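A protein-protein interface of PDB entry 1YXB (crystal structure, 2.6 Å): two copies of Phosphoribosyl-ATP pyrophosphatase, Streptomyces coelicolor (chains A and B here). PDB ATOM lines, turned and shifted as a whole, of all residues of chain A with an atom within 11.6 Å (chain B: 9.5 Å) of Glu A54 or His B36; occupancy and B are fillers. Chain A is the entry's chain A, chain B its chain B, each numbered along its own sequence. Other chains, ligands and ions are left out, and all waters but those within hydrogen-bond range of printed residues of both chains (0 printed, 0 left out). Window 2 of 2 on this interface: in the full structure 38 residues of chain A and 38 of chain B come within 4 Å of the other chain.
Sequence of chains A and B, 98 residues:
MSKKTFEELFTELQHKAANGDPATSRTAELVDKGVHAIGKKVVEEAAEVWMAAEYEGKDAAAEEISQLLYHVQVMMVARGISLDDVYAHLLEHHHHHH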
ATOM      1  N   GLU A  45      -7.982  -6.052  33.892  1.00  0.00           N
ATOM      2  CA  GLU A  45      -7.917  -5.978  32.438  1.00  0.00           C
ATOM      3  C   GLU A  45      -9.241  -5.615  31.774  1.00  0.00           C
ATOM      4  O   GLU A  45      -9.245  -4.980  30.740  1.00  0.00           O
ATOM      5  CB  GLU A  45      -7.381  -7.272  31.831  1.00  0.00           C
ATOM      6  CG  GLU A  45      -5.903  -7.557  32.096  1.00  0.00           C
ATOM      7  CD  GLU A  45      -4.950  -6.485  31.566  1.00  0.00           C
ATOM      8  OE1 GLU A  45      -5.254  -5.803  30.559  1.00  0.00           O
ATOM      9  OE2 GLU A  45      -3.865  -6.326  32.162  1.00  0.00           O
ATOM     10  N   ALA A  46     -10.353  -6.040  32.358  1.00  0.00           N
ATOM     11  CA  ALA A  46     -11.673  -5.741  31.835  1.00  0.00           C
ATOM     12  C   ALA A  46     -11.898  -4.222  31.890  1.00  0.00           C
ATOM     13  O   ALA A  46     -12.464  -3.640  30.953  1.00  0.00           O
ATOM     14  CB  ALA A  46     -12.711  -6.459  32.651  1.00  0.00           C
ATOM     15  N   ALA A  47     -11.447  -3.593  32.982  1.00  0.00           N
ATOM     16  CA  ALA A  47     -11.575  -2.160  33.149  1.00  0.00           C
ATOM     17  C   ALA A  47     -10.650  -1.440  32.191  1.00  0.00           C
ATOM     18  O   ALA A  47     -10.934  -0.323  31.774  1.00  0.00           O
ATOM     19  CB  ALA A  47     -11.255  -1.751  34.575  1.00  0.00           C
ATOM     20  N   GLU A  48      -9.519  -2.055  31.872  1.00  0.00           N
ATOM     21  CA  GLU A  48      -8.578  -1.454  30.950  1.00  0.00           C
ATOM     22  C   GLU A  48      -9.148  -1.563  29.545  1.00  0.00           C
ATOM     23  O   GLU A  48      -8.972  -0.655  28.728  1.00  0.00           O
ATOM     24  CB  GLU A  48      -7.205  -2.119  31.045  1.00  0.00           C
ATOM     25  CG  GLU A  48      -6.526  -1.915  32.397  1.00  0.00           C
ATOM     26  CD  GLU A  48      -5.066  -1.460  32.287  1.00  0.00           C
ATOM     27  OE1 GLU A  48      -4.151  -2.270  32.564  1.00  0.00           O
ATOM     28  OE2 GLU A  48      -4.829  -0.284  31.936  1.00  0.00           O
ATOM     29  N   VAL A  49      -9.816  -2.683  29.265  1.00  0.00           N
ATOM     30  CA  VAL A  49     -10.450  -2.894  27.964  1.00  0.00           C
ATOM     31  C   VAL A  49     -11.509  -1.807  27.725  1.00  0.00           C
ATOM     32  O   VAL A  49     -11.490  -1.136  26.699  1.00  0.00           O
ATOM     33  CB  VAL A  49     -11.082  -4.281  27.863  1.00  0.00           C
ATOM     34  CG1 VAL A  49     -12.075  -4.326  26.736  1.00  0.00           C
ATOM     35  CG2 VAL A  49     -10.006  -5.291  27.623  1.00  0.00           C
ATOM     36  N   TRP A  50     -12.349  -1.575  28.731  1.00  0.00           N
ATOM     37  CA  TRP A  50     -13.380  -0.563  28.642  1.00  0.00           C
ATOM     38  C   TRP A  50     -12.729   0.795  28.415  1.00  0.00           C
ATOM     39  O   TRP A  50     -13.104   1.503  27.481  1.00  0.00           O
ATOM     40  CB  TRP A  50     -14.223  -0.541  29.921  1.00  0.00           C
ATOM     41  CG  TRP A  50     -15.450   0.355  29.848  1.00  0.00           C
ATOM     42  CD1 TRP A  50     -15.885   1.076  28.762  1.00  0.00           C
ATOM     43  CD2 TRP A  50     -16.422   0.575  30.884  1.00  0.00           C
ATOM     44  NE1 TRP A  50     -17.062   1.722  29.059  1.00  0.00           N
ATOM     45  CE2 TRP A  50     -17.411   1.444  30.354  1.00  0.00           C
ATOM     46  CE3 TRP A  50     -16.539   0.155  32.213  1.00  0.00           C
ATOM     47  CZ2 TRP A  50     -18.527   1.853  31.097  1.00  0.00           C
ATOM     48  CZ3 TRP A  50     -17.646   0.567  32.951  1.00  0.00           C
ATOM     49  CH2 TRP A  50     -18.615   1.423  32.394  1.00  0.00           C
ATOM     50  N   MET A  51     -11.737   1.119  29.248  1.00  0.00           N
ATOM     51  CA  MET A  51     -11.012   2.382  29.187  1.00  0.00           C
ATOM     52  C   MET A  51     -10.438   2.662  27.809  1.00  0.00           C
ATOM     53  O   MET A  51     -10.731   3.703  27.218  1.00  0.00           O
ATOM     54  CB  MET A  51      -9.901   2.404  30.228  1.00  0.00           C
ATOM     55  CG  MET A  51      -9.775   3.741  30.844  1.00  0.00           C
ATOM     56  SD  MET A  51      -8.472   3.765  32.308  1.00  0.00           S
ATOM     57  CE  MET A  51      -9.278   2.372  33.520  1.00  0.00           C
ATOM     58  N   ALA A  52      -9.659   1.716  27.285  1.00  0.00           N
ATOM     59  CA  ALA A  52      -9.054   1.853  25.962  1.00  0.00           C
ATOM     60  C   ALA A  52     -10.122   1.954  24.872  1.00  0.00           C
ATOM     61  O   ALA A  52      -9.977   2.713  23.941  1.00  0.00           O
ATOM     62  CB  ALA A  52      -8.125   0.683  25.673  1.00  0.00           C
ATOM     63  N   ALA A  53     -11.194   1.184  25.002  1.00  0.00           N
ATOM     64  CA  ALA A  53     -12.277   1.199  24.036  1.00  0.00           C
ATOM     65  C   ALA A  53     -12.938   2.568  23.939  1.00  0.00           C
ATOM     66  O   ALA A  53     -13.416   2.962  22.877  1.00  0.00           O
ATOM     67  CB  ALA A  53     -13.312   0.176  24.424  1.00  0.00           C
ATOM     68  N   GLU A  54     -12.957   3.284  25.054  1.00  0.00           N
ATOM     69  CA  GLU A  54     -13.586   4.591  25.126  1.00  0.00           C
ATOM     70  C   GLU A  54     -12.663   5.750  24.792  1.00  0.00           C
ATOM     71  O   GLU A  54     -13.071   6.663  24.092  1.00  0.00           O
ATOM     72  CB  GLU A  54     -14.150   4.799  26.530  1.00  0.00           C
ATOM     73  CG  GLU A  54     -15.132   5.935  26.671  1.00  0.00           C
ATOM     74  CD  GLU A  54     -16.545   5.510  26.337  1.00  0.00           C
ATOM     75  OE1 GLU A  54     -17.164   4.785  27.159  1.00  0.00           O
ATOM     76  OE2 GLU A  54     -17.037   5.902  25.254  1.00  0.00           O
ATOM     77  N   TYR A  55     -11.427   5.710  25.286  1.00  0.00           N
ATOM     78  CA  TYR A  55     -10.472   6.804  25.076  1.00  0.00           C
ATOM     79  C   TYR A  55      -9.281   6.633  24.127  1.00  0.00           C
ATOM     80  O   TYR A  55      -8.666   7.624  23.714  1.00  0.00           O
ATOM     81  CB  TYR A  55      -9.923   7.248  26.425  1.00  0.00           C
ATOM     82  CG  TYR A  55     -10.959   7.818  27.340  1.00  0.00           C
ATOM     83  CD1 TYR A  55     -11.546   7.032  28.310  1.00  0.00           C
ATOM     84  CD2 TYR A  55     -11.336   9.158  27.255  1.00  0.00           C
ATOM     85  CE1 TYR A  55     -12.475   7.558  29.182  1.00  0.00           C
ATOM     86  CE2 TYR A  55     -12.268   9.689  28.128  1.00  0.00           C
ATOM     87  CZ  TYR A  55     -12.833   8.881  29.088  1.00  0.00           C
ATOM     88  OH  TYR A  55     -13.747   9.387  29.972  1.00  0.00           O
ATOM     89  N   GLU A  56      -8.927   5.399  23.805  1.00  0.00           N
ATOM     90  CA  GLU A  56      -7.777   5.163  22.952  1.00  0.00           C
ATOM     91  C   GLU A  56      -8.109   4.718  21.547  1.00  0.00           C
ATOM     92  O   GLU A  56      -9.270   4.621  21.178  1.00  0.00           O
ATOM     93  CB  GLU A  56      -6.852   4.145  23.615  1.00  0.00           C
ATOM     94  CG  GLU A  56      -6.295   4.590  24.948  1.00  0.00           C
ATOM     95  CD  GLU A  56      -5.493   5.877  24.873  1.00  0.00           C
ATOM     96  OE1 GLU A  56      -4.985   6.224  23.781  1.00  0.00           O
ATOM     97  OE2 GLU A  56      -5.348   6.533  25.930  1.00  0.00           O
ATOM     98  N   GLY A  57      -7.062   4.460  20.767  1.00  0.00           N
ATOM     99  CA  GLY A  57      -7.218   4.004  19.400  1.00  0.00           C
ATOM    100  C   GLY A  57      -7.500   2.516  19.310  1.00  0.00           C
ATOM    101  O   GLY A  57      -7.417   1.796  20.301  1.00  0.00           O
ATOM    102  N   LYS A  58      -7.830   2.052  18.111  1.00  0.00           N
ATOM    103  CA  LYS A  58      -8.146   0.651  17.898  1.00  0.00           C
ATOM    104  C   LYS A  58      -7.026  -0.294  18.315  1.00  0.00           C
ATOM    105  O   LYS A  58      -7.285  -1.315  18.949  1.00  0.00           O
ATOM    106  CB  LYS A  58      -8.536   0.413  16.439  1.00  0.00           C
ATOM    107  CG  LYS A  58      -9.905   0.952  16.077  1.00  0.00           C
ATOM    108  CD  LYS A  58     -10.148   0.959  14.565  1.00  0.00           C
ATOM    109  CE  LYS A  58     -10.015  -0.425  13.929  1.00  0.00           C
ATOM    110  NZ  LYS A  58      -8.603  -0.901  13.813  1.00  0.00           N
ATOM    111  N   ASP A  59      -5.784   0.060  17.997  1.00  0.00           N
ATOM    112  CA  ASP A  59      -4.656  -0.797  18.342  1.00  0.00           C
ATOM    113  C   ASP A  59      -4.476  -0.965  19.847  1.00  0.00           C
ATOM    114  O   ASP A  59      -4.233  -2.074  20.330  1.00  0.00           O
ATOM    115  CB  ASP A  59      -3.365  -0.292  17.715  1.00  0.00           C
ATOM    116  CG  ASP A  59      -2.210  -1.239  17.946  1.00  0.00           C
ATOM    117  OD1 ASP A  59      -2.291  -2.382  17.446  1.00  0.00           O
ATOM    118  OD2 ASP A  59      -1.247  -0.860  18.653  1.00  0.00           O
ATOM    119  N   ALA A  60      -4.556   0.147  20.574  1.00  0.00           N
ATOM    120  CA  ALA A  60      -4.451   0.135  22.031  1.00  0.00           C
ATOM    121  C   ALA A  60      -5.572  -0.717  22.645  1.00  0.00           C
ATOM    122  O   ALA A  60      -5.352  -1.449  23.605  1.00  0.00           O
ATOM    123  CB  ALA A  60      -4.520   1.533  22.560  1.00  0.00           C
ATOM    124  N   ALA A  61      -6.759  -0.661  22.055  1.00  0.00           N
ATOM    125  CA  ALA A  61      -7.880  -1.440  22.554  1.00  0.00           C
ATOM    126  C   ALA A  61      -7.635  -2.921  22.288  1.00  0.00           C
ATOM    127  O   ALA A  61      -7.929  -3.754  23.141  1.00  0.00           O
ATOM    128  CB  ALA A  61      -9.177  -0.980  21.913  1.00  0.00           C
ATOM    129  N   ALA A  62      -7.071  -3.231  21.119  1.00  0.00           N
ATOM    130  CA  ALA A  62      -6.762  -4.612  20.737  1.00  0.00           C
ATOM    131  C   ALA A  62      -5.720  -5.205  21.683  1.00  0.00           C
ATOM    132  O   ALA A  62      -5.861  -6.349  22.119  1.00  0.00           O
ATOM    133  CB  ALA A  62      -6.265  -4.672  19.316  1.00  0.00           C
ATOM    134  N   GLU A  64      -5.139  -4.332  24.812  1.00  0.00           N
ATOM    135  CA  GLU A  64      -5.759  -4.578  26.107  1.00  0.00           C
ATOM    136  C   GLU A  64      -6.688  -5.779  26.044  1.00  0.00           C
ATOM    137  O   GLU A  64      -6.816  -6.510  27.023  1.00  0.00           O
ATOM    138  CB  GLU A  64      -6.536  -3.362  26.603  1.00  0.00           C
ATOM    139  CG  GLU A  64      -5.692  -2.142  26.888  1.00  0.00           C
ATOM    140  CD  GLU A  64      -4.610  -2.381  27.924  1.00  0.00           C
ATOM    141  OE1 GLU A  64      -4.796  -3.238  28.822  1.00  0.00           O
ATOM    142  OE2 GLU A  64      -3.569  -1.688  27.840  1.00  0.00           O
ATOM    143  N   ILE A  65      -7.340  -5.982  24.900  1.00  0.00           N
ATOM    144  CA  ILE A  65      -8.240  -7.112  24.749  1.00  0.00           C
ATOM    145  C   ILE A  65      -7.451  -8.411  24.757  1.00  0.00           C
ATOM    146  O   ILE A  65      -7.890  -9.391  25.350  1.00  0.00           O
ATOM    147  CB  ILE A  65      -9.115  -7.011  23.471  1.00  0.00           C
ATOM    148  CG1 ILE A  65     -10.205  -5.970  23.669  1.00  0.00           C
ATOM    149  CG2 ILE A  65      -9.756  -8.343  23.153  1.00  0.00           C
ATOM    150  CD1 ILE A  65     -11.025  -5.702  22.431  1.00  0.00           C
ATOM    151  N   LEU B  30     -25.948  -4.464  21.016  1.00  0.00           N
ATOM    152  CA  LEU B  30     -25.269  -3.556  21.924  1.00  0.00           C
ATOM    153  C   LEU B  30     -24.414  -2.590  21.117  1.00  0.00           C
ATOM    154  O   LEU B  30     -24.116  -1.492  21.573  1.00  0.00           O
ATOM    155  CB  LEU B  30     -24.379  -4.352  22.875  1.00  0.00           C
ATOM    156  CG  LEU B  30     -25.059  -5.340  23.819  1.00  0.00           C
ATOM    157  CD1 LEU B  30     -24.282  -6.629  23.890  1.00  0.00           C
ATOM    158  CD2 LEU B  30     -25.208  -4.720  25.198  1.00  0.00           C
ATOM    159  N   VAL B  31     -24.035  -3.001  19.910  1.00  0.00           N
ATOM    160  CA  VAL B  31     -23.218  -2.166  19.036  1.00  0.00           C
ATOM    161  C   VAL B  31     -23.908  -0.833  18.803  1.00  0.00           C
ATOM    162  O   VAL B  31     -23.245   0.192  18.649  1.00  0.00           O
ATOM    163  CB  VAL B  31     -22.982  -2.837  17.678  1.00  0.00           C
ATOM    164  CG1 VAL B  31     -22.054  -1.992  16.819  1.00  0.00           C
ATOM    165  CG2 VAL B  31     -22.415  -4.225  17.876  1.00  0.00           C
ATOM    166  N   ASP B  32     -25.239  -0.854  18.791  1.00  0.00           N
ATOM    167  CA  ASP B  32     -26.018   0.358  18.589  1.00  0.00           C
ATOM    168  C   ASP B  32     -25.929   1.252  19.820  1.00  0.00           C
ATOM    169  O   ASP B  32     -25.710   2.462  19.695  1.00  0.00           O
ATOM    170  CB  ASP B  32     -27.473   0.017  18.282  1.00  0.00           C
ATOM    171  CG  ASP B  32     -28.283   1.237  17.900  1.00  0.00           C
ATOM    172  OD1 ASP B  32     -28.064   1.773  16.791  1.00  0.00           O
ATOM    173  OD2 ASP B  32     -29.134   1.663  18.709  1.00  0.00           O
ATOM    174  N   LYS B  33     -26.060   0.652  21.007  1.00  0.00           N
ATOM    175  CA  LYS B  33     -25.978   1.401  22.260  1.00  0.00           C
ATOM    176  C   LYS B  33     -24.582   1.995  22.461  1.00  0.00           C
ATOM    177  O   LYS B  33     -24.426   3.032  23.103  1.00  0.00           O
ATOM    178  CB  LYS B  33     -26.351   0.515  23.442  1.00  0.00           C
ATOM    179  CG  LYS B  33     -27.691  -0.181  23.285  1.00  0.00           C
ATOM    180  CD  LYS B  33     -28.188  -0.810  24.588  1.00  0.00           C
ATOM    181  CE  LYS B  33     -28.833   0.219  25.520  1.00  0.00           C
ATOM    182  NZ  LYS B  33     -27.877   1.232  26.056  1.00  0.00           N
ATOM    183  N   GLY B  34     -23.564   1.332  21.925  1.00  0.00           N
ATOM    184  CA  GLY B  34     -22.221   1.863  22.044  1.00  0.00           C
ATOM    185  C   GLY B  34     -21.300   1.242  23.061  1.00  0.00           C
ATOM    186  O   GLY B  34     -21.681   0.358  23.823  1.00  0.00           O
ATOM    187  N   VAL B  35     -20.084   1.780  23.083  1.00  0.00           N
ATOM    188  CA  VAL B  35     -19.001   1.337  23.959  1.00  0.00           C
ATOM    189  C   VAL B  35     -19.353   1.334  25.436  1.00  0.00           C
ATOM    190  O   VAL B  35     -19.154   0.330  26.109  1.00  0.00           O
ATOM    191  CB  VAL B  35     -17.734   2.167  23.710  1.00  0.00           C
ATOM    192  CG1 VAL B  35     -16.666   1.822  24.701  1.00  0.00           C
ATOM    193  CG2 VAL B  35     -17.229   1.896  22.324  1.00  0.00           C
ATOM    194  N   HIS B  36     -19.923   2.431  25.926  1.00  0.00           N
ATOM    195  CA  HIS B  36     -20.303   2.519  27.329  1.00  0.00           C
ATOM    196  C   HIS B  36     -21.164   1.349  27.794  1.00  0.00           C
ATOM    197  O   HIS B  36     -20.895   0.772  28.844  1.00  0.00           O
ATOM    198  CB  HIS B  36     -21.030   3.825  27.613  1.00  0.00           C
ATOM    199  CG  HIS B  36     -21.243   4.084  29.073  1.00  0.00           C
ATOM    200  ND1 HIS B  36     -20.346   4.785  29.842  1.00  0.00           N
ATOM    201  CD2 HIS B  36     -22.252   3.715  29.903  1.00  0.00           C
ATOM    202  CE1 HIS B  36     -20.788   4.842  31.090  1.00  0.00           C
ATOM    203  NE2 HIS B  36     -21.940   4.202  31.152  1.00  0.00           N
ATOM    204  N   ALA B  37     -22.183   0.987  27.015  1.00  0.00           N
ATOM    205  CA  ALA B  37     -23.064  -0.119  27.384  1.00  0.00           C
ATOM    206  C   ALA B  37     -22.368  -1.489  27.369  1.00  0.00           C
ATOM    207  O   ALA B  37     -22.643  -2.339  28.208  1.00  0.00           O
ATOM    208  CB  ALA B  37     -24.295  -0.136  26.484  1.00  0.00           C
ATOM    209  N   ILE B  38     -21.482  -1.698  26.403  1.00  0.00           N
ATOM    210  CA  ILE B  38     -20.753  -2.953  26.277  1.00  0.00           C
ATOM    211  C   ILE B  38     -19.699  -3.026  27.388  1.00  0.00           C
ATOM    212  O   ILE B  38     -19.500  -4.078  27.988  1.00  0.00           O
ATOM    213  CB  ILE B  38     -20.099  -3.056  24.896  1.00  0.00           C
ATOM    214  CG1 ILE B  38     -21.174  -2.955  23.808  1.00  0.00           C
ATOM    215  CG2 ILE B  38     -19.297  -4.334  24.789  1.00  0.00           C
ATOM    216  CD1 ILE B  38     -20.626  -2.799  22.407  1.00  0.00           C
ATOM    217  N   GLY B  39     -19.087  -1.881  27.690  1.00  0.00           N
ATOM    218  CA  GLY B  39     -18.090  -1.793  28.745  1.00  0.00           C
ATOM    219  C   GLY B  39     -18.648  -2.200  30.101  1.00  0.00           C
ATOM    220  O   GLY B  39     -17.957  -2.860  30.875  1.00  0.00           O
ATOM    221  N   LYS B  40     -19.896  -1.810  30.379  1.00  0.00           N
ATOM    222  CA  LYS B  40     -20.553  -2.166  31.636  1.00  0.00           C
ATOM    223  C   LYS B  40     -20.620  -3.680  31.721  1.00  0.00           C
ATOM    224  O   LYS B  40     -20.333  -4.265  32.754  1.00  0.00           O
ATOM    225  CB  LYS B  40     -21.986  -1.618  31.710  1.00  0.00           C
ATOM    226  CG  LYS B  40     -22.131  -0.126  31.935  1.00  0.00           C
ATOM    227  CD  LYS B  40     -23.591   0.194  32.177  1.00  0.00           C
ATOM    228  CE  LYS B  40     -23.847   1.679  32.274  1.00  0.00           C
ATOM    229  NZ  LYS B  40     -25.253   1.978  32.689  1.00  0.00           N
ATOM    230  N   LYS B  41     -21.007  -4.307  30.621  1.00  0.00           N
ATOM    231  CA  LYS B  41     -21.113  -5.750  30.578  1.00  0.00           C
ATOM    232  C   LYS B  41     -19.780  -6.460  30.733  1.00  0.00           C
ATOM    233  O   LYS B  41     -19.719  -7.452  31.430  1.00  0.00           O
ATOM    234  CB  LYS B  41     -21.800  -6.198  29.292  1.00  0.00           C
ATOM    235  CG  LYS B  41     -23.206  -5.640  29.130  1.00  0.00           C
ATOM    236  CD  LYS B  41     -24.125  -6.045  30.278  1.00  0.00           C
ATOM    237  CE  LYS B  41     -24.289  -7.546  30.356  1.00  0.00           C
ATOM    238  NZ  LYS B  41     -25.199  -7.922  31.451  1.00  0.00           N
ATOM    239  N   VAL B  42     -18.726  -5.967  30.081  1.00  0.00           N
ATOM    240  CA  VAL B  42     -17.410  -6.593  30.176  1.00  0.00           C
ATOM    241  C   VAL B  42     -16.891  -6.575  31.613  1.00  0.00           C
ATOM    242  O   VAL B  42     -16.447  -7.574  32.142  1.00  0.00           O
ATOM    243  CB  VAL B  42     -16.377  -5.920  29.228  1.00  0.00           C
ATOM    244  CG1 VAL B  42     -14.969  -6.371  29.566  1.00  0.00           C
ATOM    245  CG2 VAL B  42     -16.674  -6.295  27.753  1.00  0.00           C
ATOM    246  N   VAL B  43     -17.057  -5.436  32.249  1.00  0.00           N
ATOM    247  CA  VAL B  43     -16.645  -5.181  33.602  1.00  0.00           C
ATOM    248  C   VAL B  43     -17.469  -5.988  34.616  1.00  0.00           C
ATOM    249  O   VAL B  43     -16.926  -6.442  35.640  1.00  0.00           O
ATOM    250  CB  VAL B  43     -16.690  -3.638  33.832  1.00  0.00           C
ATOM    251  CG1 VAL B  43     -16.870  -3.262  35.264  1.00  0.00           C
ATOM    252  CG2 VAL B  43     -15.430  -3.028  33.301  1.00  0.00           C
ATOM    253  N   GLU B  44     -18.763  -6.174  34.345  1.00  0.00           N
ATOM    254  CA  GLU B  44     -19.588  -6.960  35.252  1.00  0.00           C
ATOM    255  C   GLU B  44     -19.337  -8.459  35.101  1.00  0.00           C
ATOM    256  O   GLU B  44     -19.242  -9.163  36.096  1.00  0.00           O
ATOM    257  CB  GLU B  44     -21.078  -6.616  35.154  1.00  0.00           C
ATOM    258  CG  GLU B  44     -21.795  -7.109  33.944  1.00  0.00           C
ATOM    259  CD  GLU B  44     -23.293  -7.069  34.131  1.00  0.00           C
ATOM    260  OE1 GLU B  44     -23.884  -5.985  33.950  1.00  0.00           O
ATOM    261  OE2 GLU B  44     -23.877  -8.122  34.466  1.00  0.00           O
ATOM    262  N   MET B  75     -17.423  -5.958  21.764  1.00  0.00           N
ATOM    263  CA  MET B  75     -16.644  -4.734  21.872  1.00  0.00           C
ATOM    264  C   MET B  75     -15.710  -4.638  20.661  1.00  0.00           C
ATOM    265  O   MET B  75     -15.518  -3.562  20.108  1.00  0.00           O
ATOM    266  CB  MET B  75     -15.842  -4.713  23.182  1.00  0.00           C
ATOM    267  CG  MET B  75     -14.967  -3.459  23.342  1.00  0.00           C
ATOM    268  SD  MET B  75     -16.113  -1.801  23.637  1.00  0.00           S
ATOM    269  CE  MET B  75     -16.306  -2.001  25.610  1.00  0.00           C
ATOM    270  N   ALA B  78     -17.780  -3.514  17.790  1.00  0.00           N
ATOM    271  CA  ALA B  78     -18.145  -2.119  17.978  1.00  0.00           C
ATOM    272  C   ALA B  78     -17.041  -1.124  17.695  1.00  0.00           C
ATOM    273  O   ALA B  78     -17.317   0.026  17.344  1.00  0.00           O
ATOM    274  CB  ALA B  78     -18.668  -1.916  19.370  1.00  0.00           C
ATOM    275  N   ARG B  79     -15.798  -1.568  17.836  1.00  0.00           N
ATOM    276  CA  ARG B  79     -14.632  -0.711  17.612  1.00  0.00           C
ATOM    277  C   ARG B  79     -13.885  -1.008  16.317  1.00  0.00           C
ATOM    278  O   ARG B  79     -12.840  -0.423  16.045  1.00  0.00           O
ATOM    279  CB  ARG B  79     -13.670  -0.817  18.800  1.00  0.00           C
ATOM    280  CG  ARG B  79     -14.192  -0.176  20.068  1.00  0.00           C
ATOM    281  CD  ARG B  79     -14.066   1.330  19.991  1.00  0.00           C
ATOM    282  NE  ARG B  79     -12.663   1.740  20.039  1.00  0.00           N
ATOM    283  CZ  ARG B  79     -12.139   2.695  19.282  1.00  0.00           C
ATOM    284  NH1 ARG B  79     -12.897   3.340  18.412  1.00  0.00           N
ATOM    285  NH2 ARG B  79     -10.867   3.032  19.413  1.00  0.00           N
ATOM    286  N   ILE B  81     -12.284  -3.721  15.546  1.00  0.00           N
ATOM    287  CA  ILE B  81     -11.071  -4.503  15.803  1.00  0.00           C
ATOM    288  C   ILE B  81     -11.272  -5.924  15.275  1.00  0.00           C
ATOM    289  O   ILE B  81     -12.328  -6.530  15.461  1.00  0.00           O
ATOM    290  CB  ILE B  81     -10.756  -4.575  17.320  1.00  0.00           C
ATOM    291  CG1 ILE B  81     -10.616  -3.175  17.904  1.00  0.00           C
ATOM    292  CG2 ILE B  81      -9.465  -5.334  17.561  1.00  0.00           C
ATOM    293  CD1 ILE B  81     -10.445  -3.177  19.383  1.00  0.00           C
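The guanidinium group of Arg B79 is in hydrogen-bond range of the backbone carbonyl oxygen of Ala A53 (3.2 Å). The guanidinium group of Arg B79 sits at hydrogen-bond distance from the backbone carbonyl oxygen of Glu A56 (2.9 Å). The backbone NH (N) of Lys A58 lies close to the guanidinium group (NH2) of Arg B79.
O of Ala A46 touches CG2 of Val B43 (3.8 Å). Ala A47 touches Val B43. Trp A50 touches Val B35. Trp A50 touches His B36. Gly B39 touches Trp A50 (CA to CG, 3.6 Å). Lys B40 touches Trp A50 (CG to CH2, 3.9 Å). Val B43 touches Trp A50 (CG2 to CE3, 3.5 Å). CB of Ala A53 touches CG1 of Val B35, 3.7 Å away. Glu A54 touches Val B35 (OE1 to CG1, 3.9 Å). Gly A57 touches Arg B79 (C to NH2, 3.4 Å).
Of chain B, only Val B35, Met B75 and Arg B79 come within 4 Å of Ala A53. Of the printed residues of chain B, Glu A54 touches Val B35 (3.9 Å) and His B36 (3.8 Å). No residue of chain B comes within 4 Å of Tyr A55. Val B31 touches none of the printed residues of chain A. No residue of chain A comes within 4 Å of Gly B34. Of chain A, only Trp A50, Ala A53 and Glu A54 come within 4 Å of Val B35. Of chain A, only Trp A50 and Glu A54 come within 4 Å of His B36. No residue of chain A comes within 4 Å of Ala B37. No residue of chain A comes within 4 Å of Ile B38. Of chain A, only Trp A50 comes within 4 Å of Gly B39. Of the printed residues of chain A, Val B43 touches Ala A46 (3.8 Å), Ala A47 (3.95 Å) and Trp A50 (3.5 Å). Of the printed residues of chain A, Ile B81 touches Lys A58, Ala A61 and Ala A62. The nearest printed residue of chain B that does not touch Gly A57 is Ile B81 (5.9 Å).
Hydrophobic or aromatic side chains of chain A that line the printed part of chain B: Ala A46, Trp A50, Ala A53, Ala A61 and Ala A62. Among the printed residues, no Asp or Glu carboxylate lies within 4 Å of a Lys or Arg side-chain nitrogen of the other chain.
No position is printed for both chains. Of the 19 pairs that touch across the chains among the printed residues, none has its exchanged pair printed and touching as well.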
